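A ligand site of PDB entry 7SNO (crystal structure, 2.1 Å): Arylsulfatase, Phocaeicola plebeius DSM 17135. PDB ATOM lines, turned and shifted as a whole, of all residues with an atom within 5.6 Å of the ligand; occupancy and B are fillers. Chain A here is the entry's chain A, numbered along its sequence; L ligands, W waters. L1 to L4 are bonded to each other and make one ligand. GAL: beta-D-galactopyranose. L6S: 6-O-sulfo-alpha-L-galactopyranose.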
ATOM      1  N   ASP A  40      26.898 -31.654  22.855  1.00  0.00           N
ATOM      2  CA  ASP A  40      26.099 -31.109  21.778  1.00  0.00           C
ATOM      3  C   ASP A  40      26.363 -29.610  21.606  1.00  0.00           C
ATOM      4  O   ASP A  40      26.130 -28.815  22.509  1.00  0.00           O
ATOM      5  CB  ASP A  40      24.632 -31.368  22.116  1.00  0.00           C
ATOM      6  CG  ASP A  40      23.733 -31.248  20.935  1.00  0.00           C
ATOM      7  OD1 ASP A  40      24.178 -30.658  19.933  1.00  0.00           O
ATOM      8  OD2 ASP A  40      22.597 -31.745  20.986  1.00  0.00           O
ATOM      9  N   ASP A  41      26.877 -29.206  20.431  1.00  0.00           N
ATOM     10  CA  ASP A  41      27.060 -27.794  20.092  1.00  0.00           C
ATOM     11  C   ASP A  41      28.058 -27.084  20.988  1.00  0.00           C
ATOM     12  O   ASP A  41      28.010 -25.842  21.111  1.00  0.00           O
ATOM     13  CB  ASP A  41      25.736 -27.003  20.132  1.00  0.00           C
ATOM     14  CG  ASP A  41      24.768 -27.410  19.049  1.00  0.00           C
ATOM     15  OD1 ASP A  41      25.173 -28.099  18.076  1.00  0.00           O
ATOM     16  OD2 ASP A  41      23.588 -27.048  19.163  1.00  0.00           O
ATOM     17  N   ILE A  82      26.070 -30.414  11.253  1.00  0.00           N
ATOM     18  CA  ILE A  82      24.866 -30.615  12.059  1.00  0.00           C
ATOM     19  C   ILE A  82      24.998 -31.950  12.777  1.00  0.00           C
ATOM     20  O   ILE A  82      25.840 -32.788  12.433  1.00  0.00           O
ATOM     21  CB  ILE A  82      23.566 -30.614  11.226  1.00  0.00           C
ATOM     22  CG1 ILE A  82      23.859 -30.914   9.760  1.00  0.00           C
ATOM     23  CG2 ILE A  82      22.811 -29.282  11.447  1.00  0.00           C
ATOM     24  CD1 ILE A  82      22.619 -31.096   8.926  1.00  0.00           C
ATOM     25  N   SER A  83      24.106 -32.178  13.744  1.00  0.00           N
ATOM     26  CA  SER A  83      24.292 -33.225  14.732  1.00  0.00           C
ATOM     27  C   SER A  83      24.280 -34.615  14.098  1.00  0.00           C
ATOM     28  O   SER A  83      25.272 -35.350  14.173  1.00  0.00           O
ATOM     29  CB  SER A  83      23.195 -33.113  15.800  1.00  0.00           C
ATOM     30  OG  SER A  83      23.250 -34.195  16.694  1.00  0.00           O
ATOM     31  N   THR A  84      23.173 -35.006  13.477  1.00  0.00           N
ATOM     32  CA  THR A  84      23.069 -36.364  12.952  1.00  0.00           C
ATOM     33  C   THR A  84      24.134 -36.679  11.908  1.00  0.00           C
ATOM     34  O   THR A  84      24.770 -37.749  12.004  1.00  0.00           O
ATOM     35  CB  THR A  84      21.644 -36.580  12.412  1.00  0.00           C
ATOM     36  OG1 THR A  84      20.713 -36.498  13.501  1.00  0.00           O
ATOM     37  CG2 THR A  84      21.535 -37.973  11.746  1.00  0.00           C
ATOM     38  N   LEU A 104      19.857 -33.798   8.802  1.00  0.00           N
ATOM     39  CA  LEU A 104      19.068 -34.234   9.942  1.00  0.00           C
ATOM     40  C   LEU A 104      17.879 -35.089   9.528  1.00  0.00           C
ATOM     41  O   LEU A 104      17.244 -35.693  10.399  1.00  0.00           O
ATOM     42  CB  LEU A 104      18.564 -33.017  10.737  1.00  0.00           C
ATOM     43  CG  LEU A 104      19.677 -32.176  11.371  1.00  0.00           C
ATOM     44  CD1 LEU A 104      19.229 -30.738  11.635  1.00  0.00           C
ATOM     45  CD2 LEU A 104      20.198 -32.845  12.642  1.00  0.00           C
ATOM     46  N   ASP A 105      17.562 -35.162   8.245  1.00  0.00           N
ATOM     47  CA  ASP A 105      16.404 -35.912   7.788  1.00  0.00           C
ATOM     48  C   ASP A 105      16.714 -37.386   7.569  1.00  0.00           C
ATOM     49  O   ASP A 105      15.790 -38.166   7.308  1.00  0.00           O
ATOM     50  CB  ASP A 105      15.862 -35.328   6.460  1.00  0.00           C
ATOM     51  CG  ASP A 105      15.163 -33.972   6.627  1.00  0.00           C
ATOM     52  OD1 ASP A 105      15.372 -33.116   5.719  1.00  0.00           O
ATOM     53  OD2 ASP A 105      14.454 -33.716   7.640  1.00  0.00           O
ATOM     54  N   LYS A 131      23.127 -38.568  24.457  1.00  0.00           N
ATOM     55  CA  LYS A 131      22.478 -38.234  23.186  1.00  0.00           C
ATOM     56  C   LYS A 131      23.005 -39.146  22.070  1.00  0.00           C
ATOM     57  O   LYS A 131      24.208 -39.220  21.832  1.00  0.00           O
ATOM     58  CB  LYS A 131      22.691 -36.768  22.814  1.00  0.00           C
ATOM     59  CG  LYS A 131      21.984 -36.375  21.537  1.00  0.00           C
ATOM     60  CD  LYS A 131      22.053 -34.845  21.211  1.00  0.00           C
ATOM     61  CE  LYS A 131      21.798 -34.597  19.701  1.00  0.00           C
ATOM     62  NZ  LYS A 131      21.730 -33.141  19.295  1.00  0.00           N
ATOM     63  N   HIS A 133      20.891 -39.699  18.686  1.00  0.00           N
ATOM     64  CA  HIS A 133      20.474 -38.844  17.598  1.00  0.00           C
ATOM     65  C   HIS A 133      20.845 -39.419  16.240  1.00  0.00           C
ATOM     66  O   HIS A 133      21.036 -38.661  15.270  1.00  0.00           O
ATOM     67  CB  HIS A 133      21.062 -37.447  17.755  1.00  0.00           C
ATOM     68  CG  HIS A 133      20.236 -36.383  17.097  1.00  0.00           C
ATOM     69  ND1 HIS A 133      20.707 -35.107  16.881  1.00  0.00           N
ATOM     70  CD2 HIS A 133      18.987 -36.418  16.575  1.00  0.00           C
ATOM     71  CE1 HIS A 133      19.763 -34.389  16.290  1.00  0.00           C
ATOM     72  NE2 HIS A 133      18.717 -35.164  16.088  1.00  0.00           N
ATOM     73  N   HIS A 150      11.725 -35.693  22.043  1.00  0.00           N
ATOM     74  CA  HIS A 150      11.846 -34.708  20.979  1.00  0.00           C
ATOM     75  C   HIS A 150      12.796 -35.216  19.879  1.00  0.00           C
ATOM     76  O   HIS A 150      13.766 -34.557  19.501  1.00  0.00           O
ATOM     77  CB  HIS A 150      12.280 -33.350  21.530  1.00  0.00           C
ATOM     78  CG  HIS A 150      11.358 -32.798  22.577  1.00  0.00           C
ATOM     79  ND1 HIS A 150      10.730 -33.594  23.509  1.00  0.00           N
ATOM     80  CD2 HIS A 150      10.966 -31.531  22.845  1.00  0.00           C
ATOM     81  CE1 HIS A 150       9.978 -32.837  24.299  1.00  0.00           C
ATOM     82  NE2 HIS A 150      10.108 -31.582  23.919  1.00  0.00           N
ATOM     83  N   GLY A 151      12.514 -36.432  19.410  1.00  0.00           N
ATOM     84  CA  GLY A 151      13.165 -36.992  18.238  1.00  0.00           C
ATOM     85  C   GLY A 151      14.644 -37.259  18.380  1.00  0.00           C
ATOM     86  O   GLY A 151      15.363 -37.207  17.383  1.00  0.00           O
ATOM     87  N   GLN A 153      16.711 -35.521  20.593  1.00  0.00           N
ATOM     88  CA  GLN A 153      17.336 -34.416  21.321  1.00  0.00           C
ATOM     89  C   GLN A 153      17.231 -34.589  22.829  1.00  0.00           C
ATOM     90  O   GLN A 153      18.069 -34.047  23.567  1.00  0.00           O
ATOM     91  CB  GLN A 153      16.702 -33.092  20.939  1.00  0.00           C
ATOM     92  CG  GLN A 153      16.700 -32.813  19.465  1.00  0.00           C
ATOM     93  CD  GLN A 153      18.060 -32.366  18.983  1.00  0.00           C
ATOM     94  OE1 GLN A 153      19.073 -32.667  19.618  1.00  0.00           O
ATOM     95  NE2 GLN A 153      18.096 -31.659  17.843  1.00  0.00           N
ATOM     96  N   ASP A 215      20.844 -26.072  21.475  1.00  0.00           N
ATOM     97  CA  ASP A 215      20.182 -24.801  21.150  1.00  0.00           C
ATOM     98  C   ASP A 215      19.286 -24.298  22.253  1.00  0.00           C
ATOM     99  O   ASP A 215      19.168 -23.079  22.435  1.00  0.00           O
ATOM    100  CB  ASP A 215      19.281 -24.937  19.923  1.00  0.00           C
ATOM    101  CG  ASP A 215      20.053 -24.988  18.674  1.00  0.00           C
ATOM    102  OD1 ASP A 215      20.619 -26.065  18.396  1.00  0.00           O
ATOM    103  OD2 ASP A 215      20.099 -23.952  17.992  1.00  0.00           O
ATOM    104  N   ARG A 271      13.171 -15.549  12.149  1.00  0.00           N
ATOM    105  CA  ARG A 271      13.663 -16.240  13.332  1.00  0.00           C
ATOM    106  C   ARG A 271      14.960 -15.601  13.760  1.00  0.00           C
ATOM    107  O   ARG A 271      15.961 -15.658  13.038  1.00  0.00           O
ATOM    108  CB  ARG A 271      13.856 -17.722  13.049  1.00  0.00           C
ATOM    109  CG  ARG A 271      14.410 -18.503  14.218  1.00  0.00           C
ATOM    110  CD  ARG A 271      14.738 -19.936  13.800  1.00  0.00           C
ATOM    111  NE  ARG A 271      15.252 -20.710  14.922  1.00  0.00           N
ATOM    112  CZ  ARG A 271      15.412 -22.023  14.908  1.00  0.00           C
ATOM    113  NH1 ARG A 271      15.187 -22.723  13.806  1.00  0.00           N
ATOM    114  NH2 ARG A 271      15.790 -22.638  16.016  1.00  0.00           N
ATOM    115  N   ASP A 333      29.937 -32.075  18.677  1.00  0.00           N
ATOM    116  CA  ASP A 333      29.553 -32.684  17.401  1.00  0.00           C
ATOM    117  C   ASP A 333      29.772 -31.725  16.239  1.00  0.00           C
ATOM    118  O   ASP A 333      29.960 -32.167  15.105  1.00  0.00           O
ATOM    119  CB  ASP A 333      28.110 -33.198  17.407  1.00  0.00           C
ATOM    120  CG  ASP A 333      27.085 -32.182  17.909  1.00  0.00           C
ATOM    121  OD1 ASP A 333      27.449 -31.064  18.317  1.00  0.00           O
ATOM    122  OD2 ASP A 333      25.876 -32.504  17.851  1.00  0.00           O
ATOM    123  N   GLN A 334      29.722 -30.418  16.499  1.00  0.00           N
ATOM    124  CA  GLN A 334      30.099 -29.374  15.531  1.00  0.00           C
ATOM    125  C   GLN A 334      30.265 -28.081  16.327  1.00  0.00           C
ATOM    126  O   GLN A 334      29.852 -27.990  17.493  1.00  0.00           O
ATOM    127  CB  GLN A 334      29.057 -29.172  14.413  1.00  0.00           C
ATOM    128  CG  GLN A 334      27.811 -30.030  14.519  1.00  0.00           C
ATOM    129  CD  GLN A 334      26.745 -29.472  15.446  1.00  0.00           C
ATOM    130  OE1 GLN A 334      25.663 -30.037  15.553  1.00  0.00           O
ATOM    131  NE2 GLN A 334      27.027 -28.319  16.085  1.00  0.00           N
ATOM    132  N   GLN A 344      23.604 -17.335  13.919  1.00  0.00           N
ATOM    133  CA  GLN A 344      23.416 -18.295  15.001  1.00  0.00           C
ATOM    134  C   GLN A 344      23.404 -19.722  14.454  1.00  0.00           C
ATOM    135  O   GLN A 344      23.394 -19.958  13.232  1.00  0.00           O
ATOM    136  CB  GLN A 344      22.114 -18.027  15.762  1.00  0.00           C
ATOM    137  CG  GLN A 344      20.889 -18.205  14.886  1.00  0.00           C
ATOM    138  CD  GLN A 344      19.627 -18.319  15.699  1.00  0.00           C
ATOM    139  OE1 GLN A 344      19.267 -19.412  16.138  1.00  0.00           O
ATOM    140  NE2 GLN A 344      18.950 -17.193  15.916  1.00  0.00           N
ATOM    141  N   ASP A 345      23.391 -20.683  15.382  1.00  0.00           N
ATOM    142  CA  ASP A 345      23.363 -22.113  15.066  1.00  0.00           C
ATOM    143  C   ASP A 345      24.631 -22.557  14.317  1.00  0.00           C
ATOM    144  O   ASP A 345      25.704 -21.979  14.498  1.00  0.00           O
ATOM    145  CB  ASP A 345      22.104 -22.443  14.275  1.00  0.00           C
ATOM    146  CG  ASP A 345      21.722 -23.914  14.390  1.00  0.00           C
ATOM    147  OD1 ASP A 345      21.138 -24.305  15.443  1.00  0.00           O
ATOM    148  OD2 ASP A 345      22.040 -24.686  13.447  1.00  0.00           O
ATOM    149  N   LYS A 346      24.522 -23.604  13.514  1.00  0.00           N
ATOM    150  CA  LYS A 346      25.727 -24.133  12.878  1.00  0.00           C
ATOM    151  C   LYS A 346      25.532 -24.226  11.364  1.00  0.00           C
ATOM    152  O   LYS A 346      25.140 -23.246  10.722  1.00  0.00           O
ATOM    153  CB  LYS A 346      26.113 -25.476  13.506  1.00  0.00           C
ATOM    154  CG  LYS A 346      24.977 -26.467  13.709  1.00  0.00           C
ATOM    155  CD  LYS A 346      24.274 -26.230  15.054  1.00  0.00           C
ATOM    156  CE  LYS A 346      23.233 -27.283  15.318  1.00  0.00           C
ATOM    157  NZ  LYS A 346      22.335 -26.901  16.424  1.00  0.00           N
ATOM    158  N   ARG A 347      25.841 -25.373  10.755  1.00  0.00           N
ATOM    159  CA  ARG A 347      25.531 -25.584   9.343  1.00  0.00           C
ATOM    160  C   ARG A 347      26.505 -24.853   8.414  1.00  0.00           C
ATOM    161  O   ARG A 347      26.925 -25.408   7.391  1.00  0.00           O
ATOM    162  CB  ARG A 347      24.090 -25.173   9.051  1.00  0.00           C
ATOM    163  CG  ARG A 347      23.078 -26.003   9.826  1.00  0.00           C
ATOM    164  CD  ARG A 347      21.741 -25.261  10.000  1.00  0.00           C
ATOM    165  NE  ARG A 347      20.899 -25.878  11.026  1.00  0.00           N
ATOM    166  CZ  ARG A 347      19.933 -26.756  10.799  1.00  0.00           C
ATOM    167  NH1 ARG A 347      19.676 -27.215   9.579  1.00  0.00           N
ATOM    168  NH2 ARG A 347      19.192 -27.193  11.809  1.00  0.00           N
ATOM    169  N   ILE A 427      16.679 -25.589   5.138  1.00  0.00           N
ATOM    170  CA  ILE A 427      15.771 -26.061   6.178  1.00  0.00           C
ATOM    171  C   ILE A 427      16.233 -25.588   7.550  1.00  0.00           C
ATOM    172  O   ILE A 427      17.433 -25.605   7.856  1.00  0.00           O
ATOM    173  CB  ILE A 427      15.649 -27.593   6.135  1.00  0.00           C
ATOM    174  CG1 ILE A 427      14.859 -28.018   4.907  1.00  0.00           C
ATOM    175  CG2 ILE A 427      14.982 -28.129   7.436  1.00  0.00           C
ATOM    176  CD1 ILE A 427      15.337 -29.320   4.338  1.00  0.00           C
ATOM    177  N   HIS A 428      15.276 -25.126   8.368  1.00  0.00           N
ATOM    178  CA  HIS A 428      15.496 -24.805   9.797  1.00  0.00           C
ATOM    179  C   HIS A 428      16.088 -23.429  10.048  1.00  0.00           C
ATOM    180  O   HIS A 428      15.641 -22.714  10.966  1.00  0.00           O
ATOM    181  CB  HIS A 428      16.415 -25.829  10.471  1.00  0.00           C
ATOM    182  CG  HIS A 428      15.829 -27.197  10.588  1.00  0.00           C
ATOM    183  ND1 HIS A 428      16.609 -28.327  10.695  1.00  0.00           N
ATOM    184  CD2 HIS A 428      14.539 -27.619  10.617  1.00  0.00           C
ATOM    185  CE1 HIS A 428      15.824 -29.386  10.798  1.00  0.00           C
ATOM    186  NE2 HIS A 428      14.565 -28.991  10.741  1.00  0.00           N
ATOM    187  N   HIS A 429      17.134 -23.057   9.307  1.00  0.00           N
ATOM    188  CA  HIS A 429      17.842 -21.812   9.610  1.00  0.00           C
ATOM    189  C   HIS A 429      18.139 -20.995   8.368  1.00  0.00           C
ATOM    190  O   HIS A 429      18.934 -20.042   8.434  1.00  0.00           O
ATOM    191  CB  HIS A 429      19.143 -22.142  10.383  1.00  0.00           C
ATOM    192  CG  HIS A 429      18.932 -22.320  11.855  1.00  0.00           C
ATOM    193  ND1 HIS A 429      18.683 -21.257  12.695  1.00  0.00           N
ATOM    194  CD2 HIS A 429      18.938 -23.429  12.630  1.00  0.00           C
ATOM    195  CE1 HIS A 429      18.541 -21.704  13.935  1.00  0.00           C
ATOM    196  NE2 HIS A 429      18.679 -23.019  13.922  1.00  0.00           N
ATOM    197  N   ARG A 456      11.420 -31.041  -2.172  1.00  0.00           N
ATOM    198  CA  ARG A 456      11.423 -30.118  -1.046  1.00  0.00           C
ATOM    199  C   ARG A 456      11.146 -28.689  -1.492  1.00  0.00           C
ATOM    200  O   ARG A 456      10.635 -27.896  -0.698  1.00  0.00           O
ATOM    201  CB  ARG A 456      12.756 -30.203  -0.303  1.00  0.00           C
ATOM    202  CG  ARG A 456      12.982 -31.467   0.524  1.00  0.00           C
ATOM    203  CD  ARG A 456      11.715 -31.906   1.261  1.00  0.00           C
ATOM    204  NE  ARG A 456      11.585 -31.249   2.556  1.00  0.00           N
ATOM    205  CZ  ARG A 456      12.358 -31.463   3.610  1.00  0.00           C
ATOM    206  NH1 ARG A 456      13.363 -32.339   3.573  1.00  0.00           N
ATOM    207  NH2 ARG A 456      12.121 -30.803   4.746  1.00  0.00           N
ATOM    208  N   SER A 461      10.753 -23.798   5.062  1.00  0.00           N
ATOM    209  CA  SER A 461      12.036 -24.110   5.688  1.00  0.00           C
ATOM    210  C   SER A 461      11.859 -24.390   7.173  1.00  0.00           C
ATOM    211  O   SER A 461      12.590 -25.210   7.730  1.00  0.00           O
ATOM    212  CB  SER A 461      13.046 -22.977   5.483  1.00  0.00           C
ATOM    213  OG  SER A 461      12.581 -21.755   6.045  1.00  0.00           O
ATOM    214  N   SER A 463       8.860 -25.518   9.386  1.00  0.00           N
ATOM    215  CA  SER A 463       7.501 -25.974   9.147  1.00  0.00           C
ATOM    216  C   SER A 463       6.562 -25.723  10.313  1.00  0.00           C
ATOM    217  O   SER A 463       5.346 -25.858  10.136  1.00  0.00           O
ATOM    218  CB  SER A 463       7.507 -27.460   8.776  1.00  0.00           C
ATOM    219  OG  SER A 463       8.054 -28.211   9.822  1.00  0.00           O
ATOM    220  N   TRP A 464       7.076 -25.339  11.487  1.00  0.00           N
ATOM    221  CA  TRP A 464       6.190 -24.949  12.584  1.00  0.00           C
ATOM    222  C   TRP A 464       5.732 -23.507  12.509  1.00  0.00           C
ATOM    223  O   TRP A 464       5.026 -23.070  13.410  1.00  0.00           O
ATOM    224  CB  TRP A 464       6.893 -25.175  13.931  1.00  0.00           C
ATOM    225  CG  TRP A 464       8.134 -24.372  14.060  1.00  0.00           C
ATOM    226  CD1 TRP A 464       8.269 -23.162  14.639  1.00  0.00           C
ATOM    227  CD2 TRP A 464       9.434 -24.723  13.547  1.00  0.00           C
ATOM    228  NE1 TRP A 464       9.577 -22.731  14.555  1.00  0.00           N
ATOM    229  CE2 TRP A 464      10.304 -23.680  13.883  1.00  0.00           C
ATOM    230  CE3 TRP A 464       9.938 -25.819  12.843  1.00  0.00           C
ATOM    231  CZ2 TRP A 464      11.657 -23.687  13.545  1.00  0.00           C
ATOM    232  CZ3 TRP A 464      11.270 -25.846  12.516  1.00  0.00           C
ATOM    233  CH2 TRP A 464      12.114 -24.791  12.858  1.00  0.00           C
HETATM  234  C1  GAL L   1       3.788 -32.738  16.116  1.00  0.00           C
HETATM  235  C2  GAL L   1       5.226 -32.496  15.629  1.00  0.00           C
HETATM  236  C3  GAL L   1       6.176 -31.761  16.611  1.00  0.00           C
HETATM  237  C4  GAL L   1       5.438 -30.516  17.091  1.00  0.00           C
HETATM  238  C5  GAL L   1       4.199 -31.101  17.797  1.00  0.00           C
HETATM  239  C6  GAL L   1       3.524 -30.101  18.709  1.00  0.00           C
HETATM  240  O1  GAL L   1       2.996 -33.052  14.959  1.00  0.00           O
HETATM  241  O2  GAL L   1       5.779 -33.731  15.139  1.00  0.00           O
HETATM  242  O3  GAL L   1       7.310 -31.575  15.765  1.00  0.00           O
HETATM  243  O4  GAL L   1       5.023 -29.623  16.060  1.00  0.00           O
HETATM  244  O5  GAL L   1       3.287 -31.586  16.797  1.00  0.00           O
HETATM  245  O6  GAL L   1       4.423 -29.828  19.781  1.00  0.00           O
HETATM  246  O1S L6S L   2      12.292 -31.310  10.437  1.00  0.00           O
HETATM  247  O2S L6S L   2      11.775 -29.130  11.039  1.00  0.00           O
HETATM  248  O3S L6S L   2      10.081 -30.394   9.656  1.00  0.00           O
HETATM  249  C1  L6S L   2       8.324 -30.770  16.367  1.00  0.00           C
HETATM  250  C2  L6S L   2       9.354 -31.598  17.105  1.00  0.00           C
HETATM  251  C3  L6S L   2      10.162 -32.512  16.184  1.00  0.00           C
HETATM  252  C4  L6S L   2      10.632 -31.695  14.977  1.00  0.00           C
HETATM  253  C5  L6S L   2       9.503 -30.912  14.305  1.00  0.00           C
HETATM  254  C6  L6S L   2       9.982 -30.101  13.106  1.00  0.00           C
HETATM  255  O2  L6S L   2       8.757 -32.362  18.169  1.00  0.00           O
HETATM  256  O3  L6S L   2      11.233 -33.061  16.965  1.00  0.00           O
HETATM  257  O4  L6S L   2      11.602 -30.763  15.456  1.00  0.00           O
HETATM  258  O5  L6S L   2       8.888 -30.038  15.265  1.00  0.00           O
HETATM  259  O6  L6S L   2      10.569 -30.973  12.132  1.00  0.00           O
HETATM  260  S1  L6S L   2      11.214 -30.438  10.832  1.00  0.00           S
HETATM  261  C1  GAL L   3      12.889 -30.887  14.840  1.00  0.00           C
HETATM  262  C2  GAL L   3      13.562 -29.567  15.213  1.00  0.00           C
HETATM  263  C3  GAL L   3      15.027 -29.424  14.817  1.00  0.00           C
HETATM  264  C4  GAL L   3      15.783 -30.627  15.407  1.00  0.00           C
HETATM  265  C5  GAL L   3      15.090 -31.883  14.890  1.00  0.00           C
HETATM  266  C6  GAL L   3      15.585 -33.257  15.358  1.00  0.00           C
HETATM  267  O2  GAL L   3      12.834 -28.435  14.750  1.00  0.00           O
HETATM  268  O3  GAL L   3      15.512 -28.154  15.265  1.00  0.00           O
HETATM  269  O4  GAL L   3      15.794 -30.760  16.811  1.00  0.00           O
HETATM  270  O5  GAL L   3      13.706 -31.935  15.298  1.00  0.00           O
HETATM  271  O6  GAL L   3      16.898 -33.512  14.858  1.00  0.00           O
HETATM  272  O1S L6S L   4      22.493 -30.192  17.184  1.00  0.00           O
HETATM  273  O2S L6S L   4      22.124 -30.529  14.908  1.00  0.00           O
HETATM  274  O3S L6S L   4      20.593 -31.747  16.493  1.00  0.00           O
HETATM  275  C1  L6S L   4      16.339 -27.616  14.217  1.00  0.00           C
HETATM  276  C2  L6S L   4      16.710 -26.191  14.591  1.00  0.00           C
HETATM  277  C3  L6S L   4      17.460 -26.105  15.910  1.00  0.00           C
HETATM  278  C4  L6S L   4      18.705 -26.950  15.701  1.00  0.00           C
HETATM  279  C5  L6S L   4      18.296 -28.343  15.259  1.00  0.00           C
HETATM  280  C6  L6S L   4      19.505 -29.267  15.056  1.00  0.00           C
HETATM  281  O2  L6S L   4      15.530 -25.404  14.571  1.00  0.00           O
HETATM  282  O3  L6S L   4      17.740 -24.738  16.182  1.00  0.00           O
HETATM  283  O4  L6S L   4      19.521 -26.364  14.710  1.00  0.00           O
HETATM  284  O5  L6S L   4      17.529 -28.383  14.043  1.00  0.00           O
HETATM  285  O6  L6S L   4      20.491 -29.208  16.106  1.00  0.00           O
HETATM  286  S1  L6S L   4      21.463 -30.416  16.195  1.00  0.00           S
HETATM  287  O   HOH W   1      10.911 -27.386   9.013  1.00  0.00           O
HETATM  288  O   HOH W   2      13.368 -26.160  16.346  1.00  0.00           O
HETATM  289  O   HOH W   3       6.580 -28.981  12.857  1.00  0.00           O
HETATM  290  O   HOH W   4      15.071 -32.839  10.136  1.00  0.00           O
HETATM  291  O   HOH W   5      13.348 -31.517   7.371  1.00  0.00           O
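O3S of L6S L2 sits at hydrogen-bond distance from OG of Ser 463, 3.0 Å away.
O2S of L6S L4 lies within hydrogen-bond range of N of Ser 83, at 2.8 Å.
O3 of L6S L4 is in hydrogen-bond range of OD2 of Asp 215 (3.1 Å).
O2S of L6S L2 sits at hydrogen-bond distance from NE2 of His 428, 2.8 Å away.
O6 of GAL L3 is in hydrogen-bond range of NE2 of His 133, at 2.7 Å.
An oxygen (O3S) of L6S L4 is in salt-bridge range of the side-chain amino group (NZ) of Lys 131, 3.3 Å away.
An oxygen (O4) of L6S L4 sits at hydrogen-bond distance from the side-chain carboxylate (OD1) of Asp 345 (2.7 Å).
NZ of Lys 346 is in salt-bridge range of O1S of L6S L4 (3.4 Å).
O5 of L6S L4 lies within hydrogen-bond range of NH2 of Arg 347 (3.0 Å).
An oxygen (O2) of L6S L4 sits at hydrogen-bond distance from the guanidinium group (NH1) of Arg 271.
A ring nitrogen (NE2) of His 429 sits at hydrogen-bond distance from an oxygen (O3) of L6S L4, 3.0 Å away.
NE2 of Gln 153 lies within hydrogen-bond range of O4 of GAL L3.
Water W1 lies within hydrogen-bond range of the backbone NH (N) of Ser 463 (2.8 Å), an oxygen (O2S) of L6S L2 (2.8 Å) and the backbone carbonyl oxygen (O) of Ser 461 (3.0 Å).
Water W4 lies within hydrogen-bond range of OD2 of Asp 105 (2.7 Å) and O1S of L6S L2 (3.2 Å).
Water W5 lies within hydrogen-bond range of OD2 of Asp 105, NH2 of Arg 456 and O1S of L6S L2.
Water W3 bridges OG of Ser 463 (3.5 Å) and O5 of L6S L2 (3.5 Å).
NH1 of Arg 271 lies within hydrogen-bond range of O of His 428.
A ring nitrogen (ND1) of His 428 sits at hydrogen-bond distance from the guanidinium group of Arg 347 (3.0 Å).
OE1 of Gln 153 sits at hydrogen-bond distance from NZ of Lys 131 (2.7 Å).
The side-chain carboxylate of Asp 333 sits at hydrogen-bond distance from the side-chain hydroxyl of Ser 83, 3.3 Å away.
A ring nitrogen (ND1) of His 133 lies within hydrogen-bond range of the side-chain hydroxyl (OG) of Ser 83 (2.7 Å).
The side-chain carboxylate (OD2) of Asp 333 lies close to the side-chain amide oxygen (OE1) of Gln 334 (3.4 Å).
NZ of Lys 346 is in salt-bridge range of OD2 of Asp 41 (3.0 Å).
The side-chain amino group (NZ) of Lys 346 lies within salt-bridge range of the side-chain carboxylate (OD1) of Asp 345, at 3.0 Å.
OD1 of Asp 40 sits close to O1S of L6S L4 (3.3 Å).
OD1 of Asp 41 touches O1S of L6S L4 (3.5 Å).
CG2 of Ile 82 touches O2S of L6S L4 (3.7 Å).
Leu 104 touches the ligand.
His 150 touches the ligand.
Gln 334 touches the ligand.
Trp 464 touches the ligand.
Hydrophobic or aromatic side chains that line the ligand: Ile 82, Leu 104, His 133, His 428, His 429 and Trp 464.
Of the 27 residues printed, 19 come within 4 Å of the ligand.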
